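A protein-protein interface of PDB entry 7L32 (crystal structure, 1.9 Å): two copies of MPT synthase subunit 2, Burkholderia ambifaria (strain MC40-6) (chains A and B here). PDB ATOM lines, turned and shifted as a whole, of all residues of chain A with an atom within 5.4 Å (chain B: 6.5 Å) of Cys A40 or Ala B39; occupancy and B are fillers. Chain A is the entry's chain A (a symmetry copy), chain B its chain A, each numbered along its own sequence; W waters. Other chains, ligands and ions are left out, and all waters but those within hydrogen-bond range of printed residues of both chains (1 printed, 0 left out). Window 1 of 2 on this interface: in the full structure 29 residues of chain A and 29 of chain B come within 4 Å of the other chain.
The backbone carbonyl oxygen (O) of Ala B37 lies within hydrogen-bond range of the backbone NH (N) of Ala B108, at 2.9 Å. The backbone carbonyl oxygen of Ala B39 sits at hydrogen-bond distance from the backbone NH of Thr B106, 2.8 Å away. The backbone NH (N) of Phe B41 sits at hydrogen-bond distance from the backbone carbonyl oxygen (O) of Val B104 (2.8 Å). N of Thr A106 lies within hydrogen-bond range of O of Ala A39 (2.8 Å). The backbone carbonyl oxygen (O) of Val A104 lies within hydrogen-bond range of the backbone NH (N) of Phe A41 (2.8 Å). O of Val A104 lies within hydrogen-bond range of SG of Cys A118 (3.6 Å).
O of Leu B38 sits at hydrogen-bond distance from N of Val A42 (2.9 Å). The side-chain sulfur of Cys A40 forms a disulfide with the side-chain sulfur of Cys B40, at 2.1 Å. The backbone NH (N) of Val B42 sits at hydrogen-bond distance from the backbone carbonyl oxygen (O) of Leu A38 (2.9 Å).
Leu A38 touches Phe B41, and with the chains exchanged Phe A41 touches Leu B38. Leu A38 touches Val B42, and with the chains exchanged Val A42 touches Leu B38. Ala A39 touches Cys B40, and with the chains exchanged Cys A40 touches Ala B39. Cys B40 touches its own counterpart, Cys A40. Positions printed for both chains: 21, 25, 38, 39, 40, 41, 42, 104, 105, 106 and 118.
Printed residues of chain B within 4 Å of Cys A40: Ala B39 (3.5 Å) and Cys B40 (2.1 Å). Thr A106 touches none of the printed residues of chain B. Printed residues of chain A within 4 Å of Ala B37: Phe A41 (3.7 Å). Of the printed residues of chain A, Leu B38 touches Phe A41 (3.2 Å) and Val A42 (2.9 Å). Printed residues of chain A within 4 Å of Ala B39: Cys A40. The nearest printed residue of chain B that does not touch Cys A40 is Leu B38 (4.1 Å). The nearest printed residue of chain B that does not touch Leu A38 is Cys B40 (4.1 Å).
Leu A38 touches Phe B41. Cys B40 touches Ala A39 (O to CA, 3.5 Å). Cys A40 touches Ala B39 (O to CA, 3.5 Å). CB of Ala B37 touches CZ of Phe A41 (3.7 Å). CD1 of Phe A41 touches O of Leu B38 (3.2 Å). CE1 of Phe A41 touches CB of Arg B111, at 3.5 Å. Phe B115 touches Phe A41 (CZ to CB, 3.6 Å). CE1 of Phe B115 touches SG of Cys A118, at 3.8 Å.
Water W1 bridges the backbone carbonyl oxygen of Cys A40 (3.1 Å) and the backbone carbonyl oxygen of Cys B40 (3.1 Å).
Hydrophobic or aromatic side chains of chain B within 4 Å of the printed part of chain A: Ala B37, Leu B38, Phe B41 and Phe B115. Printed residues of chain A that touch a printed residue of chain B: Leu A38, Ala A39, Cys A40, Phe A41, Val A42 and Cys A118. Hydrophobic or aromatic side chains of chain A that line the printed part of chain B: Leu A38 and Phe A41. Among the printed residues, 11 pairs touch across the chains. Among the printed residues, no Asp or Glu carboxylate lies within 4 Å of a Lys or Arg side-chain nitrogen of the other chain.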
ATOM      1  N   LEU A  21      29.710 -10.714 -13.719  1.00  0.00           N
ATOM      2  CA  LEU A  21      28.451 -10.100 -13.299  1.00  0.00           C
ATOM      3  C   LEU A  21      28.647  -8.645 -12.870  1.00  0.00           C
ATOM      4  O   LEU A  21      27.884  -7.765 -13.285  1.00  0.00           O
ATOM      5  CB  LEU A  21      27.824 -10.911 -12.160  1.00  0.00           C
ATOM      6  CG  LEU A  21      26.483 -10.408 -11.608  1.00  0.00           C
ATOM      7  CD1 LEU A  21      25.379 -10.410 -12.677  1.00  0.00           C
ATOM      8  CD2 LEU A  21      26.063 -11.250 -10.422  1.00  0.00           C
ATOM      9  N   VAL A  25      26.872  -5.470 -14.616  1.00  0.00           N
ATOM     10  CA  VAL A  25      25.976  -4.645 -13.811  1.00  0.00           C
ATOM     11  C   VAL A  25      26.422  -3.187 -13.832  1.00  0.00           C
ATOM     12  O   VAL A  25      25.602  -2.280 -14.020  1.00  0.00           O
ATOM     13  CB  VAL A  25      25.896  -5.218 -12.382  1.00  0.00           C
ATOM     14  CG1 VAL A  25      25.454  -4.163 -11.364  1.00  0.00           C
ATOM     15  CG2 VAL A  25      24.966  -6.409 -12.381  1.00  0.00           C
ATOM     16  N   LEU A  38      18.098  -2.555  -9.235  1.00  0.00           N
ATOM     17  CA  LEU A  38      18.683  -3.505 -10.187  1.00  0.00           C
ATOM     18  C   LEU A  38      18.373  -4.933  -9.759  1.00  0.00           C
ATOM     19  O   LEU A  38      18.706  -5.335  -8.642  1.00  0.00           O
ATOM     20  CB  LEU A  38      20.199  -3.258 -10.294  1.00  0.00           C
ATOM     21  CG  LEU A  38      20.945  -4.172 -11.271  1.00  0.00           C
ATOM     22  CD1 LEU A  38      21.931  -3.368 -12.131  1.00  0.00           C
ATOM     23  CD2 LEU A  38      21.700  -5.135 -10.403  1.00  0.00           C
ATOM     24  N   ALA A  39      17.732  -5.706 -10.636  1.00  0.00           N
ATOM     25  CA  ALA A  39      17.487  -7.116 -10.379  1.00  0.00           C
ATOM     26  C   ALA A  39      18.309  -7.939 -11.359  1.00  0.00           C
ATOM     27  O   ALA A  39      18.404  -7.589 -12.540  1.00  0.00           O
ATOM     28  CB  ALA A  39      16.005  -7.480 -10.538  1.00  0.00           C
ATOM     29  N   CYS A  40      18.893  -9.034 -10.880  1.00  0.00           N
ATOM     30  CA  CYS A  40      19.645  -9.866 -11.804  1.00  0.00           C
ATOM     31  C   CYS A  40      19.413 -11.341 -11.508  1.00  0.00           C
ATOM     32  O   CYS A  40      18.931 -11.746 -10.438  1.00  0.00           O
ATOM     33  CB  CYS A  40      21.142  -9.515 -11.787  1.00  0.00           C
ATOM     34  SG  CYS A  40      21.948  -9.619 -10.183  1.00  0.00           S
ATOM     35  N   PHE A  41      19.693 -12.139 -12.530  1.00  0.00           N
ATOM     36  CA  PHE A  41      19.589 -13.579 -12.396  1.00  0.00           C
ATOM     37  C   PHE A  41      20.811 -14.174 -13.067  1.00  0.00           C
ATOM     38  O   PHE A  41      21.189 -13.730 -14.152  1.00  0.00           O
ATOM     39  CB  PHE A  41      18.312 -14.161 -13.018  1.00  0.00           C
ATOM     40  CG  PHE A  41      18.239 -15.675 -12.896  1.00  0.00           C
ATOM     41  CD1 PHE A  41      17.704 -16.268 -11.757  1.00  0.00           C
ATOM     42  CD2 PHE A  41      18.767 -16.498 -13.904  1.00  0.00           C
ATOM     43  CE1 PHE A  41      17.677 -17.652 -11.619  1.00  0.00           C
ATOM     44  CE2 PHE A  41      18.729 -17.889 -13.779  1.00  0.00           C
ATOM     45  CZ  PHE A  41      18.189 -18.466 -12.649  1.00  0.00           C
ATOM     46  N   VAL A  42      21.431 -15.158 -12.418  1.00  0.00           N
ATOM     47  CA  VAL A  42      22.517 -15.927 -13.017  1.00  0.00           C
ATOM     48  C   VAL A  42      22.182 -17.404 -12.898  1.00  0.00           C
ATOM     49  O   VAL A  42      21.997 -17.917 -11.787  1.00  0.00           O
ATOM     50  CB  VAL A  42      23.876 -15.643 -12.355  1.00  0.00           C
ATOM     51  CG1 VAL A  42      24.962 -16.517 -12.987  1.00  0.00           C
ATOM     52  CG2 VAL A  42      24.238 -14.164 -12.502  1.00  0.00           C
ATOM     53  N   VAL A 104      20.836 -12.361 -16.705  1.00  0.00           N
ATOM     54  CA  VAL A 104      19.889 -11.336 -17.122  1.00  0.00           C
ATOM     55  C   VAL A 104      19.889 -10.283 -16.024  1.00  0.00           C
ATOM     56  O   VAL A 104      19.802 -10.636 -14.844  1.00  0.00           O
ATOM     57  CB  VAL A 104      18.471 -11.896 -17.325  1.00  0.00           C
ATOM     58  CG1 VAL A 104      17.489 -10.728 -17.585  1.00  0.00           C
ATOM     59  CG2 VAL A 104      18.458 -12.889 -18.524  1.00  0.00           C
ATOM     60  N   ALA A 105      20.052  -9.018 -16.401  1.00  0.00           N
ATOM     61  CA  ALA A 105      19.984  -7.914 -15.435  1.00  0.00           C
ATOM     62  C   ALA A 105      19.010  -6.861 -15.956  1.00  0.00           C
ATOM     63  O   ALA A 105      18.998  -6.555 -17.154  1.00  0.00           O
ATOM     64  CB  ALA A 105      21.363  -7.289 -15.215  1.00  0.00           C
ATOM     65  N   THR A 106      18.184  -6.309 -15.061  1.00  0.00           N
ATOM     66  CA  THR A 106      17.262  -5.245 -15.422  1.00  0.00           C
ATOM     67  C   THR A 106      17.414  -4.122 -14.411  1.00  0.00           C
ATOM     68  O   THR A 106      17.779  -4.360 -13.260  1.00  0.00           O
ATOM     69  CB  THR A 106      15.795  -5.697 -15.453  1.00  0.00           C
ATOM     70  OG1 THR A 106      15.374  -6.120 -14.138  1.00  0.00           O
ATOM     71  CG2 THR A 106      15.574  -6.848 -16.472  1.00  0.00           C
ATOM     72  N   CYS A 118      12.805  -8.864 -14.965  1.00  0.00           N
ATOM     73  CA  CYS A 118      13.898  -9.833 -14.989  1.00  0.00           C
ATOM     74  C   CYS A 118      13.359 -11.258 -15.062  1.00  0.00           C
ATOM     75  O   CYS A 118      13.855 -12.086 -15.851  1.00  0.00           O
ATOM     76  CB  CYS A 118      14.785  -9.652 -13.755  1.00  0.00           C
ATOM     77  SG  CYS A 118      16.343 -10.568 -13.824  1.00  0.00           S
ATOM     78  N   LEU B  21      29.359  -7.330  -5.037  1.00  0.00           N
ATOM     79  CA  LEU B  21      28.308  -8.272  -5.423  1.00  0.00           C
ATOM     80  C   LEU B  21      28.889  -9.617  -5.864  1.00  0.00           C
ATOM     81  O   LEU B  21      28.413 -10.672  -5.431  1.00  0.00           O
ATOM     82  CB  LEU B  21      27.448  -7.671  -6.540  1.00  0.00           C
ATOM     83  CG  LEU B  21      26.284  -8.531  -7.054  1.00  0.00           C
ATOM     84  CD1 LEU B  21      25.255  -8.830  -5.954  1.00  0.00           C
ATOM     85  CD2 LEU B  21      25.613  -7.844  -8.224  1.00  0.00           C
ATOM     86  N   VAL B  25      28.118 -13.152  -4.080  1.00  0.00           N
ATOM     87  CA  VAL B  25      27.464 -14.198  -4.862  1.00  0.00           C
ATOM     88  C   VAL B  25      28.299 -15.473  -4.860  1.00  0.00           C
ATOM     89  O   VAL B  25      27.769 -16.573  -4.653  1.00  0.00           O
ATOM     90  CB  VAL B  25      27.186 -13.676  -6.285  1.00  0.00           C
ATOM     91  CG1 VAL B  25      27.026 -14.816  -7.295  1.00  0.00           C
ATOM     92  CG2 VAL B  25      25.962 -12.790  -6.255  1.00  0.00           C
ATOM     93  N   LEU B  28      27.941 -17.251  -1.507  1.00  0.00           N
ATOM     94  CA  LEU B  28      26.645 -17.923  -1.392  1.00  0.00           C
ATOM     95  C   LEU B  28      26.631 -19.230  -2.185  1.00  0.00           C
ATOM     96  O   LEU B  28      26.147 -20.259  -1.695  1.00  0.00           O
ATOM     97  CB  LEU B  28      25.512 -16.995  -1.856  1.00  0.00           C
ATOM     98  CG  LEU B  28      24.091 -17.552  -1.708  1.00  0.00           C
ATOM     99  CD1 LEU B  28      23.802 -17.851  -0.229  1.00  0.00           C
ATOM    100  CD2 LEU B  28      22.995 -16.621  -2.297  1.00  0.00           C
ATOM    101  N   ALA B  37      20.390 -21.796  -9.339  1.00  0.00           N
ATOM    102  CA  ALA B  37      19.597 -20.659  -9.805  1.00  0.00           C
ATOM    103  C   ALA B  37      19.785 -19.545  -8.792  1.00  0.00           C
ATOM    104  O   ALA B  37      19.430 -19.723  -7.626  1.00  0.00           O
ATOM    105  CB  ALA B  37      18.120 -21.029  -9.926  1.00  0.00           C
ATOM    106  N   LEU B  38      20.348 -18.415  -9.216  1.00  0.00           N
ATOM    107  CA  LEU B  38      20.674 -17.336  -8.277  1.00  0.00           C
ATOM    108  C   LEU B  38      19.966 -16.052  -8.690  1.00  0.00           C
ATOM    109  O   LEU B  38      20.142 -15.578  -9.813  1.00  0.00           O
ATOM    110  CB  LEU B  38      22.201 -17.151  -8.215  1.00  0.00           C
ATOM    111  CG  LEU B  38      22.692 -16.063  -7.256  1.00  0.00           C
ATOM    112  CD1 LEU B  38      23.886 -16.556  -6.429  1.00  0.00           C
ATOM    113  CD2 LEU B  38      23.123 -14.930  -8.142  1.00  0.00           C
ATOM    114  N   ALA B  39      19.162 -15.485  -7.792  1.00  0.00           N
ATOM    115  CA  ALA B  39      18.527 -14.199  -8.035  1.00  0.00           C
ATOM    116  C   ALA B  39      19.115 -13.175  -7.077  1.00  0.00           C
ATOM    117  O   ALA B  39      19.339 -13.481  -5.901  1.00  0.00           O
ATOM    118  CB  ALA B  39      17.008 -14.262  -7.832  1.00  0.00           C
ATOM    119  N   CYS B  40      19.357 -11.963  -7.568  1.00  0.00           N
ATOM    120  CA  CYS B  40      19.876 -10.951  -6.663  1.00  0.00           C
ATOM    121  C   CYS B  40      19.233  -9.601  -6.945  1.00  0.00           C
ATOM    122  O   CYS B  40      18.627  -9.350  -8.000  1.00  0.00           O
ATOM    123  CB  CYS B  40      21.410 -10.872  -6.724  1.00  0.00           C
ATOM    124  SG  CYS B  40      22.108 -10.555  -8.351  1.00  0.00           S
ATOM    125  N   PHE B  41      19.311  -8.752  -5.929  1.00  0.00           N
ATOM    126  CA  PHE B  41      18.806  -7.398  -6.054  1.00  0.00           C
ATOM    127  C   PHE B  41      19.833  -6.485  -5.416  1.00  0.00           C
ATOM    128  O   PHE B  41      20.352  -6.802  -4.344  1.00  0.00           O
ATOM    129  CB  PHE B  41      17.437  -7.191  -5.392  1.00  0.00           C
ATOM    130  CG  PHE B  41      16.942  -5.759  -5.506  1.00  0.00           C
ATOM    131  CD1 PHE B  41      16.230  -5.342  -6.627  1.00  0.00           C
ATOM    132  CD2 PHE B  41      17.249  -4.817  -4.510  1.00  0.00           C
ATOM    133  CE1 PHE B  41      15.815  -4.021  -6.758  1.00  0.00           C
ATOM    134  CE2 PHE B  41      16.822  -3.492  -4.629  1.00  0.00           C
ATOM    135  CZ  PHE B  41      16.111  -3.092  -5.740  1.00  0.00           C
ATOM    136  N   VAL B  42      20.136  -5.369  -6.080  1.00  0.00           N
ATOM    137  CA  VAL B  42      20.982  -4.326  -5.509  1.00  0.00           C
ATOM    138  C   VAL B  42      20.246  -3.001  -5.612  1.00  0.00           C
ATOM    139  O   VAL B  42      19.894  -2.565  -6.714  1.00  0.00           O
ATOM    140  CB  VAL B  42      22.347  -4.224  -6.212  1.00  0.00           C
ATOM    141  CG1 VAL B  42      23.165  -3.080  -5.607  1.00  0.00           C
ATOM    142  CG2 VAL B  42      23.110  -5.544  -6.080  1.00  0.00           C
ATOM    143  N   VAL B 104      20.467  -8.203  -1.787  1.00  0.00           N
ATOM    144  CA  VAL B 104      19.856  -9.450  -1.347  1.00  0.00           C
ATOM    145  C   VAL B 104      20.117 -10.466  -2.450  1.00  0.00           C
ATOM    146  O   VAL B 104      19.901 -10.156  -3.626  1.00  0.00           O
ATOM    147  CB  VAL B 104      18.344  -9.307  -1.101  1.00  0.00           C
ATOM    148  CG1 VAL B 104      17.733 -10.698  -0.817  1.00  0.00           C
ATOM    149  CG2 VAL B 104      18.091  -8.350   0.101  1.00  0.00           C
ATOM    150  N   ALA B 105      20.635 -11.634  -2.083  1.00  0.00           N
ATOM    151  CA  ALA B 105      20.850 -12.718  -3.051  1.00  0.00           C
ATOM    152  C   ALA B 105      20.222 -13.997  -2.507  1.00  0.00           C
ATOM    153  O   ALA B 105      20.331 -14.290  -1.308  1.00  0.00           O
ATOM    154  CB  ALA B 105      22.341 -12.935  -3.313  1.00  0.00           C
ATOM    155  N   THR B 106      19.557 -14.761  -3.378  1.00  0.00           N
ATOM    156  CA  THR B 106      18.978 -16.038  -2.996  1.00  0.00           C
ATOM    157  C   THR B 106      19.406 -17.079  -4.015  1.00  0.00           C
ATOM    158  O   THR B 106      19.657 -16.754  -5.176  1.00  0.00           O
ATOM    159  CB  THR B 106      17.444 -16.013  -2.920  1.00  0.00           C
ATOM    160  OG1 THR B 106      16.884 -15.727  -4.221  1.00  0.00           O
ATOM    161  CG2 THR B 106      16.942 -14.963  -1.891  1.00  0.00           C
ATOM    162  N   VAL B 107      19.518 -18.322  -3.574  1.00  0.00           N
ATOM    163  CA  VAL B 107      19.821 -19.426  -4.479  1.00  0.00           C
ATOM    164  C   VAL B 107      18.806 -20.531  -4.236  1.00  0.00           C
ATOM    165  O   VAL B 107      18.331 -20.730  -3.109  1.00  0.00           O
ATOM    166  CB  VAL B 107      21.280 -19.937  -4.328  1.00  0.00           C
ATOM    167  CG1 VAL B 107      21.586 -20.443  -2.899  1.00  0.00           C
ATOM    168  CG2 VAL B 107      21.598 -21.022  -5.364  1.00  0.00           C
ATOM    169  N   ALA B 108      18.455 -21.237  -5.315  1.00  0.00           N
ATOM    170  CA  ALA B 108      17.494 -22.316  -5.258  1.00  0.00           C
ATOM    171  C   ALA B 108      17.808 -23.290  -6.384  1.00  0.00           C
ATOM    172  O   ALA B 108      18.624 -23.016  -7.269  1.00  0.00           O
ATOM    173  CB  ALA B 108      16.058 -21.789  -5.391  1.00  0.00           C
ATOM    174  N   ARG B 111      14.571 -21.317 -10.879  1.00  0.00           N
ATOM    175  CA  ARG B 111      14.517 -19.854 -10.894  1.00  0.00           C
ATOM    176  C   ARG B 111      13.253 -19.315 -10.232  1.00  0.00           C
ATOM    177  O   ARG B 111      13.302 -18.234  -9.624  1.00  0.00           O
ATOM    178  CB  ARG B 111      14.652 -19.309 -12.334  1.00  0.00           C
ATOM    179  CG  ARG B 111      13.526 -19.674 -13.289  1.00  0.00           C
ATOM    180  CD  ARG B 111      13.750 -19.061 -14.718  1.00  0.00           C
ATOM    181  NE  ARG B 111      12.628 -19.401 -15.582  1.00  0.00           N
ATOM    182  CZ  ARG B 111      12.487 -20.567 -16.198  1.00  0.00           C
ATOM    183  NH1 ARG B 111      13.417 -21.512 -16.113  1.00  0.00           N
ATOM    184  NH2 ARG B 111      11.386 -20.794 -16.912  1.00  0.00           N
ATOM    185  N   ALA B 114      13.895 -18.890  -6.563  1.00  0.00           N
ATOM    186  CA  ALA B 114      14.918 -17.875  -6.351  1.00  0.00           C
ATOM    187  C   ALA B 114      14.343 -16.466  -6.492  1.00  0.00           C
ATOM    188  O   ALA B 114      14.532 -15.619  -5.609  1.00  0.00           O
ATOM    189  CB  ALA B 114      16.093 -18.097  -7.310  1.00  0.00           C
ATOM    190  N   PHE B 115      13.624 -16.193  -7.593  1.00  0.00           N
ATOM    191  CA  PHE B 115      13.032 -14.866  -7.793  1.00  0.00           C
ATOM    192  C   PHE B 115      12.027 -14.517  -6.695  1.00  0.00           C
ATOM    193  O   PHE B 115      12.045 -13.405  -6.154  1.00  0.00           O
ATOM    194  CB  PHE B 115      12.303 -14.801  -9.136  1.00  0.00           C
ATOM    195  CG  PHE B 115      13.194 -14.507 -10.295  1.00  0.00           C
ATOM    196  CD1 PHE B 115      13.887 -13.295 -10.366  1.00  0.00           C
ATOM    197  CD2 PHE B 115      13.299 -15.422 -11.336  1.00  0.00           C
ATOM    198  CE1 PHE B 115      14.699 -12.997 -11.472  1.00  0.00           C
ATOM    199  CE2 PHE B 115      14.097 -15.142 -12.440  1.00  0.00           C
ATOM    200  CZ  PHE B 115      14.789 -13.936 -12.521  1.00  0.00           C
ATOM    201  N   ALA B 116      11.122 -15.439  -6.381  1.00  0.00           N
ATOM    202  CA  ALA B 116      10.055 -15.127  -5.424  1.00  0.00           C
ATOM    203  C   ALA B 116      10.639 -14.813  -4.055  1.00  0.00           C
ATOM    204  O   ALA B 116      10.237 -13.841  -3.393  1.00  0.00           O
ATOM    205  CB  ALA B 116       9.064 -16.289  -5.333  1.00  0.00           C
ATOM    206  N   SER B 117      11.588 -15.634  -3.609  1.00  0.00           N
ATOM    207  CA  SER B 117      12.158 -15.423  -2.279  1.00  0.00           C
ATOM    208  C   SER B 117      12.968 -14.135  -2.224  1.00  0.00           C
ATOM    209  O   SER B 117      12.953 -13.432  -1.205  1.00  0.00           O
ATOM    210  CB  SER B 117      13.015 -16.628  -1.861  1.00  0.00           C
ATOM    211  OG  SER B 117      14.119 -16.861  -2.740  1.00  0.00           O
ATOM    212  N   CYS B 118      13.678 -13.803  -3.308  1.00  0.00           N
ATOM    213  CA  CYS B 118      14.460 -12.568  -3.312  1.00  0.00           C
ATOM    214  C   CYS B 118      13.548 -11.350  -3.217  1.00  0.00           C
ATOM    215  O   CYS B 118      13.816 -10.412  -2.440  1.00  0.00           O
ATOM    216  CB  CYS B 118      15.325 -12.501  -4.572  1.00  0.00           C
ATOM    217  SG  CYS B 118      16.569 -11.188  -4.545  1.00  0.00           S
HETATM  218  O   HOH W   1      16.218 -10.913  -9.180  1.00  0.00           O
